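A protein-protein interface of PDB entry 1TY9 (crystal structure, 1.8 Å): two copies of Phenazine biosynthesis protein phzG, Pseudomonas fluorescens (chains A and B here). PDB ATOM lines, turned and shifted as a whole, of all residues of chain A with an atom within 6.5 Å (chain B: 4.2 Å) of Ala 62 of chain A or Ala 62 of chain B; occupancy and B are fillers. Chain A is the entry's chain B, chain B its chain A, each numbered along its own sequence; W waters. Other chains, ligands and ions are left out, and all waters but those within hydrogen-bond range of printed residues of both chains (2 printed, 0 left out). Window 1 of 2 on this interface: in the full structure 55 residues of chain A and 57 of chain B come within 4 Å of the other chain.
Ala 62 of chain A touches three residues of chain B.
Printed residues of chain B within 4 Å of Ser 106 of chain A: Pro 70 (3.2 Å), Ser 71 (3.6 Å) and Thr 72 (2.8 Å).
Of the printed residues of chain B, Ser 71 of chain A touches Ser 106 (3.5 Å).
Of the printed residues of chain A, Ala 60 of chain B touches Ala 60 and Val 108.
Printed residues of chain A within 4 Å of Ala 105 of chain B: Pro 70 (3.95 Å).
The nearest printed residue of chain B that does not touch Ala 62 of chain A is Ser 71 of chain B (5.0 Å).
The nearest residue of chain A that does not touch Ala 62 of chain B is Ser 71 of chain A (4.9 Å).
The nearest printed residue of chain A that does not touch Ala 105 of chain B is Ser 71 of chain A (5.9 Å).
The side-chain hydroxyl (OG1) of Thr 72 of chain B is in hydrogen-bond range of the side-chain hydroxyl (OG) of Ser 106 of chain A (2.8 Å).
OG of Ser 106 of chain B is in hydrogen-bond range of OG1 of Thr 72 of chain A.
Of the 16 printed residues of chain A, 11 touch a printed residue of chain B.
Hydrophobic or aromatic side chains of chain A within 4 Å of the printed part of chain B: Ala 60, Ala 62, Pro 70 and Val 108.
Of the 9 printed residues of chain B, 8 touch a printed residue of chain A.
Printed residues of chain B that touch a printed residue of chain A: Ala 60, Ala 62, Thr 63, Pro 70, Ser 71, Thr 72, Ala 105 and Ser 106.
Ala 62 of chain A touches Ala 62 of chain B (CB to CB, 3.4 Å).
Ala 62 of chain A touches Pro 70 of chain B.
Ala 62 of chain A touches Thr 72 of chain B (CB to CG2, 3.5 Å).
CG of Pro 70 of chain A touches O of Ala 62 of chain B, at 3.8 Å.
Pro 70 of chain A touches Thr 63 of chain B.
Pro 70 of chain A touches Ala 105 of chain B.
Ser 106 of chain B touches Ser 71 of chain A.
Thr 72 of chain B touches Gly 107 of chain A (OG1 to C, 3.5 Å).
Ala 60 of chain B touches Val 108 of chain A.
Thr 72 of chain B touches Val 108 of chain A (OG1 to N, 3.6 Å).
Water W1 lies within hydrogen-bond range of O of Pro 70 of chain B (2.8 Å) and O of Ala 105 of chain A (3.0 Å).
Water W2 bridges the backbone carbonyl oxygen of Pro 70 of chain A and the backbone carbonyl oxygen of Ala 105 of chain B.
Ala 62 of chain B touches its own counterpart, Ala 62 of chain A.
Ala 62 of chain A touches Pro 70 of chain B, and with the chains exchanged Pro 70 of chain A touches Ala 62 of chain B.
Ala 62 of chain A touches Thr 72 of chain B, and with the chains exchanged Thr 72 of chain A touches Ala 62 of chain B.
Thr 63 of chain A touches Pro 70 of chain B, and with the chains exchanged Pro 70 of chain A touches Thr 63 of chain B.
9 positions are printed for both chains.
The backbone NH (N) of Ala 62 of chain A lies within hydrogen-bond range of the backbone carbonyl oxygen (O) of Ser 106 of chain A, 2.7 Å away.
OG1 of Thr 63 of chain A is in hydrogen-bond range of NH1 of Arg 73 of chain A.
The backbone carbonyl oxygen (O) of Thr 63 of chain B is in hydrogen-bond range of the backbone NH (N) of Ser 71 of chain B, at 2.9 Å.
The backbone NH (N) of Ser 71 of chain A is in hydrogen-bond range of the backbone carbonyl oxygen (O) of Thr 63 of chain A (2.9 Å).
OE1 of Glu 98 of chain A lies within hydrogen-bond range of OG of Ser 71 of chain A, at 2.8 Å.
The side-chain hydroxyl of Thr 63 of chain A is in hydrogen-bond range of the side-chain carboxylate of Glu 98 of chain A.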
ATOM      1  N   ALA A  60     -24.470  23.588   9.508  1.00  0.00           N
ATOM      2  CA  ALA A  60     -25.110  24.379  10.510  1.00  0.00           C
ATOM      3  C   ALA A  60     -23.958  24.996  11.305  1.00  0.00           C
ATOM      4  O   ALA A  60     -23.337  24.323  12.071  1.00  0.00           O
ATOM      5  CB  ALA A  60     -25.996  23.490  11.412  1.00  0.00           C
ATOM      6  N   LEU A  61     -23.709  26.298  11.135  1.00  0.00           N
ATOM      7  CA  LEU A  61     -22.493  26.889  11.629  1.00  0.00           C
ATOM      8  C   LEU A  61     -22.815  27.680  12.880  1.00  0.00           C
ATOM      9  O   LEU A  61     -23.678  28.549  12.790  1.00  0.00           O
ATOM     10  CB  LEU A  61     -21.948  27.853  10.583  1.00  0.00           C
ATOM     11  CG  LEU A  61     -20.792  28.763  10.984  1.00  0.00           C
ATOM     12  CD1 LEU A  61     -19.584  27.852  11.007  1.00  0.00           C
ATOM     13  CD2 LEU A  61     -20.594  29.821   9.916  1.00  0.00           C
ATOM     14  N   ALA A  62     -22.088  27.436  13.982  1.00  0.00           N
ATOM     15  CA  ALA A  62     -22.224  28.195  15.261  1.00  0.00           C
ATOM     16  C   ALA A  62     -21.045  29.133  15.452  1.00  0.00           C
ATOM     17  O   ALA A  62     -19.900  28.756  15.201  1.00  0.00           O
ATOM     18  CB  ALA A  62     -22.272  27.201  16.490  1.00  0.00           C
ATOM     19  N   THR A  63     -21.365  30.367  15.829  1.00  0.00           N
ATOM     20  CA  THR A  63     -20.389  31.338  16.289  1.00  0.00           C
ATOM     21  C   THR A  63     -20.939  31.795  17.657  1.00  0.00           C
ATOM     22  O   THR A  63     -22.000  31.317  18.090  1.00  0.00           O
ATOM     23  CB  THR A  63     -20.313  32.519  15.247  1.00  0.00           C
ATOM     24  OG1 THR A  63     -21.633  32.985  14.964  1.00  0.00           O
ATOM     25  CG2 THR A  63     -19.870  31.978  13.844  1.00  0.00           C
ATOM     26  N   ALA A  64     -20.206  32.677  18.332  1.00  0.00           N
ATOM     27  CA  ALA A  64     -20.538  33.114  19.668  1.00  0.00           C
ATOM     28  C   ALA A  64     -20.302  34.628  19.784  1.00  0.00           C
ATOM     29  O   ALA A  64     -19.385  35.200  19.173  1.00  0.00           O
ATOM     30  CB  ALA A  64     -19.652  32.403  20.702  1.00  0.00           C
ATOM     31  N   PRO A  70     -23.965  31.357  22.000  1.00  0.00           N
ATOM     32  CA  PRO A  70     -23.952  30.847  20.602  1.00  0.00           C
ATOM     33  C   PRO A  70     -25.085  31.396  19.742  1.00  0.00           C
ATOM     34  O   PRO A  70     -26.180  31.720  20.227  1.00  0.00           O
ATOM     35  CB  PRO A  70     -24.138  29.309  20.763  1.00  0.00           C
ATOM     36  CG  PRO A  70     -23.779  28.996  22.167  1.00  0.00           C
ATOM     37  CD  PRO A  70     -24.193  30.277  22.985  1.00  0.00           C
ATOM     38  N   SER A  71     -24.839  31.445  18.444  1.00  0.00           N
ATOM     39  CA  SER A  71     -25.873  31.632  17.445  1.00  0.00           C
ATOM     40  C   SER A  71     -25.625  30.647  16.293  1.00  0.00           C
ATOM     41  O   SER A  71     -24.505  30.197  16.103  1.00  0.00           O
ATOM     42  CB  SER A  71     -25.860  33.067  16.920  1.00  0.00           C
ATOM     43  OG  SER A  71     -24.651  33.333  16.161  1.00  0.00           O
ATOM     44  N   THR A  72     -26.653  30.338  15.526  1.00  0.00           N
ATOM     45  CA  THR A  72     -26.512  29.350  14.415  1.00  0.00           C
ATOM     46  C   THR A  72     -27.334  29.730  13.196  1.00  0.00           C
ATOM     47  O   THR A  72     -28.317  30.476  13.299  1.00  0.00           O
ATOM     48  CB  THR A  72     -27.024  27.918  14.816  1.00  0.00           C
ATOM     49  OG1 THR A  72     -28.376  28.016  15.290  1.00  0.00           O
ATOM     50  CG2 THR A  72     -26.287  27.296  16.004  1.00  0.00           C
ATOM     51  N   ARG A  73     -26.911  29.173  12.048  1.00  0.00           N
ATOM     52  CA  ARG A  73     -27.603  29.280  10.746  1.00  0.00           C
ATOM     53  C   ARG A  73     -26.911  28.297   9.813  1.00  0.00           C
ATOM     54  O   ARG A  73     -25.842  27.813  10.112  1.00  0.00           O
ATOM     55  CB  ARG A  73     -27.490  30.738  10.190  1.00  0.00           C
ATOM     56  CG  ARG A  73     -26.111  31.141   9.637  1.00  0.00           C
ATOM     57  CD  ARG A  73     -24.986  31.058  10.670  1.00  0.00           C
ATOM     58  NE  ARG A  73     -25.194  32.159  11.588  1.00  0.00           N
ATOM     59  CZ  ARG A  73     -24.504  32.386  12.698  1.00  0.00           C
ATOM     60  NH1 ARG A  73     -23.597  31.489  13.127  1.00  0.00           N
ATOM     61  NH2 ARG A  73     -24.748  33.529  13.404  1.00  0.00           N
ATOM     62  N   GLU A  98     -19.649  38.367  14.768  1.00  0.00           N
ATOM     63  CA  GLU A  98     -19.200  37.475  15.809  1.00  0.00           C
ATOM     64  C   GLU A  98     -17.797  36.923  15.514  1.00  0.00           C
ATOM     65  O   GLU A  98     -16.950  36.882  16.435  1.00  0.00           O
ATOM     66  CB  GLU A  98     -20.251  36.378  16.143  1.00  0.00           C
ATOM     67  CG  GLU A  98     -21.422  36.958  16.946  1.00  0.00           C
ATOM     68  CD  GLU A  98     -22.536  35.984  17.350  1.00  0.00           C
ATOM     69  OE1 GLU A  98     -22.448  34.771  17.099  1.00  0.00           O
ATOM     70  OE2 GLU A  98     -23.556  36.433  17.917  1.00  0.00           O
ATOM     71  N   LEU A  99     -17.530  36.533  14.262  1.00  0.00           N
ATOM     72  CA  LEU A  99     -16.228  35.911  13.917  1.00  0.00           C
ATOM     73  C   LEU A  99     -15.101  36.891  14.009  1.00  0.00           C
ATOM     74  O   LEU A  99     -13.969  36.517  14.314  1.00  0.00           O
ATOM     75  CB  LEU A  99     -16.264  35.244  12.548  1.00  0.00           C
ATOM     76  CG  LEU A  99     -17.046  33.884  12.555  1.00  0.00           C
ATOM     77  CD1 LEU A  99     -17.326  33.476  11.083  1.00  0.00           C
ATOM     78  CD2 LEU A  99     -16.283  32.808  13.396  1.00  0.00           C
ATOM     79  N   TRP A 104     -13.343  31.622  16.975  1.00  0.00           N
ATOM     80  CA  TRP A 104     -13.806  30.249  17.203  1.00  0.00           C
ATOM     81  C   TRP A 104     -15.228  29.890  16.741  1.00  0.00           C
ATOM     82  O   TRP A 104     -16.183  30.573  16.985  1.00  0.00           O
ATOM     83  CB  TRP A 104     -13.624  29.866  18.671  1.00  0.00           C
ATOM     84  CG  TRP A 104     -12.130  29.638  19.043  1.00  0.00           C
ATOM     85  CD1 TRP A 104     -11.299  30.539  19.643  1.00  0.00           C
ATOM     86  CD2 TRP A 104     -11.359  28.429  18.887  1.00  0.00           C
ATOM     87  NE1 TRP A 104     -10.047  30.001  19.818  1.00  0.00           N
ATOM     88  CE2 TRP A 104     -10.064  28.687  19.429  1.00  0.00           C
ATOM     89  CE3 TRP A 104     -11.647  27.140  18.431  1.00  0.00           C
ATOM     90  CZ2 TRP A 104      -9.040  27.709  19.494  1.00  0.00           C
ATOM     91  CZ3 TRP A 104     -10.586  26.157  18.441  1.00  0.00           C
ATOM     92  CH2 TRP A 104      -9.287  26.487  18.971  1.00  0.00           C
ATOM     93  N   ALA A 105     -15.369  28.732  16.107  1.00  0.00           N
ATOM     94  CA  ALA A 105     -16.630  28.309  15.493  1.00  0.00           C
ATOM     95  C   ALA A 105     -16.719  26.775  15.428  1.00  0.00           C
ATOM     96  O   ALA A 105     -15.719  26.063  15.574  1.00  0.00           O
ATOM     97  CB  ALA A 105     -16.769  28.883  14.047  1.00  0.00           C
ATOM     98  N   SER A 106     -17.932  26.296  15.231  1.00  0.00           N
ATOM     99  CA  SER A 106     -18.147  24.878  15.091  1.00  0.00           C
ATOM    100  C   SER A 106     -19.304  24.695  14.075  1.00  0.00           C
ATOM    101  O   SER A 106     -20.327  25.404  14.169  1.00  0.00           O
ATOM    102  CB  SER A 106     -18.577  24.320  16.456  1.00  0.00           C
ATOM    103  OG  SER A 106     -18.833  22.930  16.251  1.00  0.00           O
ATOM    104  N   GLY A 107     -19.167  23.741  13.154  1.00  0.00           N
ATOM    105  CA  GLY A 107     -20.286  23.400  12.274  1.00  0.00           C
ATOM    106  C   GLY A 107     -20.571  21.930  12.213  1.00  0.00           C
ATOM    107  O   GLY A 107     -19.666  21.136  12.318  1.00  0.00           O
ATOM    108  N   VAL A 108     -21.850  21.564  12.050  1.00  0.00           N
ATOM    109  CA  VAL A 108     -22.154  20.143  11.859  1.00  0.00           C
ATOM    110  C   VAL A 108     -22.890  19.929  10.528  1.00  0.00           C
ATOM    111  O   VAL A 108     -23.771  20.737  10.121  1.00  0.00           O
ATOM    112  CB  VAL A 108     -22.952  19.560  13.059  1.00  0.00           C
ATOM    113  CG1 VAL A 108     -24.226  20.455  13.374  1.00  0.00           C
ATOM    114  CG2 VAL A 108     -23.355  18.085  12.815  1.00  0.00           C
ATOM    115  N   ALA B  60     -29.599  21.058  15.002  1.00  0.00           N
ATOM    116  CA  ALA B  60     -28.171  21.301  15.196  1.00  0.00           C
ATOM    117  C   ALA B  60     -27.970  22.217  16.374  1.00  0.00           C
ATOM    118  O   ALA B  60     -28.149  23.422  16.244  1.00  0.00           O
ATOM    119  CB  ALA B  60     -27.540  21.905  13.939  1.00  0.00           C
ATOM    120  N   LEU B  61     -27.541  21.651  17.500  1.00  0.00           N
ATOM    121  CA  LEU B  61     -27.522  22.372  18.748  1.00  0.00           C
ATOM    122  C   LEU B  61     -26.106  22.822  19.103  1.00  0.00           C
ATOM    123  O   LEU B  61     -25.207  21.994  19.235  1.00  0.00           O
ATOM    124  CB  LEU B  61     -28.073  21.495  19.874  1.00  0.00           C
ATOM    125  CG  LEU B  61     -27.943  22.107  21.272  1.00  0.00           C
ATOM    126  CD1 LEU B  61     -29.102  23.118  21.363  1.00  0.00           C
ATOM    127  CD2 LEU B  61     -28.007  20.962  22.323  1.00  0.00           C
ATOM    128  N   ALA B  62     -25.937  24.137  19.272  1.00  0.00           N
ATOM    129  CA  ALA B  62     -24.683  24.778  19.596  1.00  0.00           C
ATOM    130  C   ALA B  62     -24.665  25.186  21.074  1.00  0.00           C
ATOM    131  O   ALA B  62     -25.638  25.750  21.554  1.00  0.00           O
ATOM    132  CB  ALA B  62     -24.570  26.103  18.750  1.00  0.00           C
ATOM    133  N   THR B  63     -23.568  24.889  21.751  1.00  0.00           N
ATOM    134  CA  THR B  63     -23.287  25.299  23.117  1.00  0.00           C
ATOM    135  C   THR B  63     -21.866  25.872  23.046  1.00  0.00           C
ATOM    136  O   THR B  63     -21.258  25.886  21.973  1.00  0.00           O
ATOM    137  CB  THR B  63     -23.305  24.054  24.082  1.00  0.00           C
ATOM    138  OG1 THR B  63     -22.368  23.066  23.617  1.00  0.00           O
ATOM    139  CG2 THR B  63     -24.662  23.358  24.164  1.00  0.00           C
ATOM    140  N   PRO B  70     -17.533  27.606  20.490  1.00  0.00           N
ATOM    141  CA  PRO B  70     -18.730  26.792  20.232  1.00  0.00           C
ATOM    142  C   PRO B  70     -18.436  25.311  19.917  1.00  0.00           C
ATOM    143  O   PRO B  70     -17.368  24.997  19.394  1.00  0.00           O
ATOM    144  CB  PRO B  70     -19.316  27.414  18.963  1.00  0.00           C
ATOM    145  CG  PRO B  70     -18.842  28.789  18.923  1.00  0.00           C
ATOM    146  CD  PRO B  70     -17.383  28.670  19.466  1.00  0.00           C
ATOM    147  N   SER B  71     -19.428  24.462  20.192  1.00  0.00           N
ATOM    148  CA  SER B  71     -19.432  23.069  19.780  1.00  0.00           C
ATOM    149  C   SER B  71     -20.836  22.771  19.239  1.00  0.00           C
ATOM    150  O   SER B  71     -21.777  23.394  19.663  1.00  0.00           O
ATOM    151  CB  SER B  71     -19.049  22.158  20.944  1.00  0.00           C
ATOM    152  OG  SER B  71     -20.002  22.181  21.987  1.00  0.00           O
ATOM    153  N   THR B  72     -20.972  21.798  18.340  1.00  0.00           N
ATOM    154  CA  THR B  72     -22.289  21.481  17.765  1.00  0.00           C
ATOM    155  C   THR B  72     -22.449  20.004  17.693  1.00  0.00           C
ATOM    156  O   THR B  72     -21.459  19.268  17.777  1.00  0.00           O
ATOM    157  CB  THR B  72     -22.444  22.048  16.344  1.00  0.00           C
ATOM    158  OG1 THR B  72     -21.287  21.688  15.583  1.00  0.00           O
ATOM    159  CG2 THR B  72     -22.431  23.673  16.401  1.00  0.00           C
ATOM    160  N   ALA B 105     -27.487  28.758  24.561  1.00  0.00           N
ATOM    161  CA  ALA B 105     -27.399  27.785  23.471  1.00  0.00           C
ATOM    162  C   ALA B 105     -28.159  28.333  22.255  1.00  0.00           C
ATOM    163  O   ALA B 105     -28.952  29.254  22.398  1.00  0.00           O
ATOM    164  CB  ALA B 105     -27.936  26.381  23.909  1.00  0.00           C
ATOM    165  N   SER B 106     -27.913  27.769  21.069  1.00  0.00           N
ATOM    166  CA  SER B 106     -28.650  28.151  19.880  1.00  0.00           C
ATOM    167  C   SER B 106     -28.777  26.831  19.095  1.00  0.00           C
ATOM    168  O   SER B 106     -27.877  25.978  19.161  1.00  0.00           O
ATOM    169  CB  SER B 106     -27.917  29.192  19.080  1.00  0.00           C
ATOM    170  OG  SER B 106     -28.573  29.412  17.846  1.00  0.00           O
HETATM  171  O   HOH W   1     -15.007  26.068  18.439  1.00  0.00           O
HETATM  172  O   HOH W   2     -27.571  31.871  22.700  1.00  0.00           O
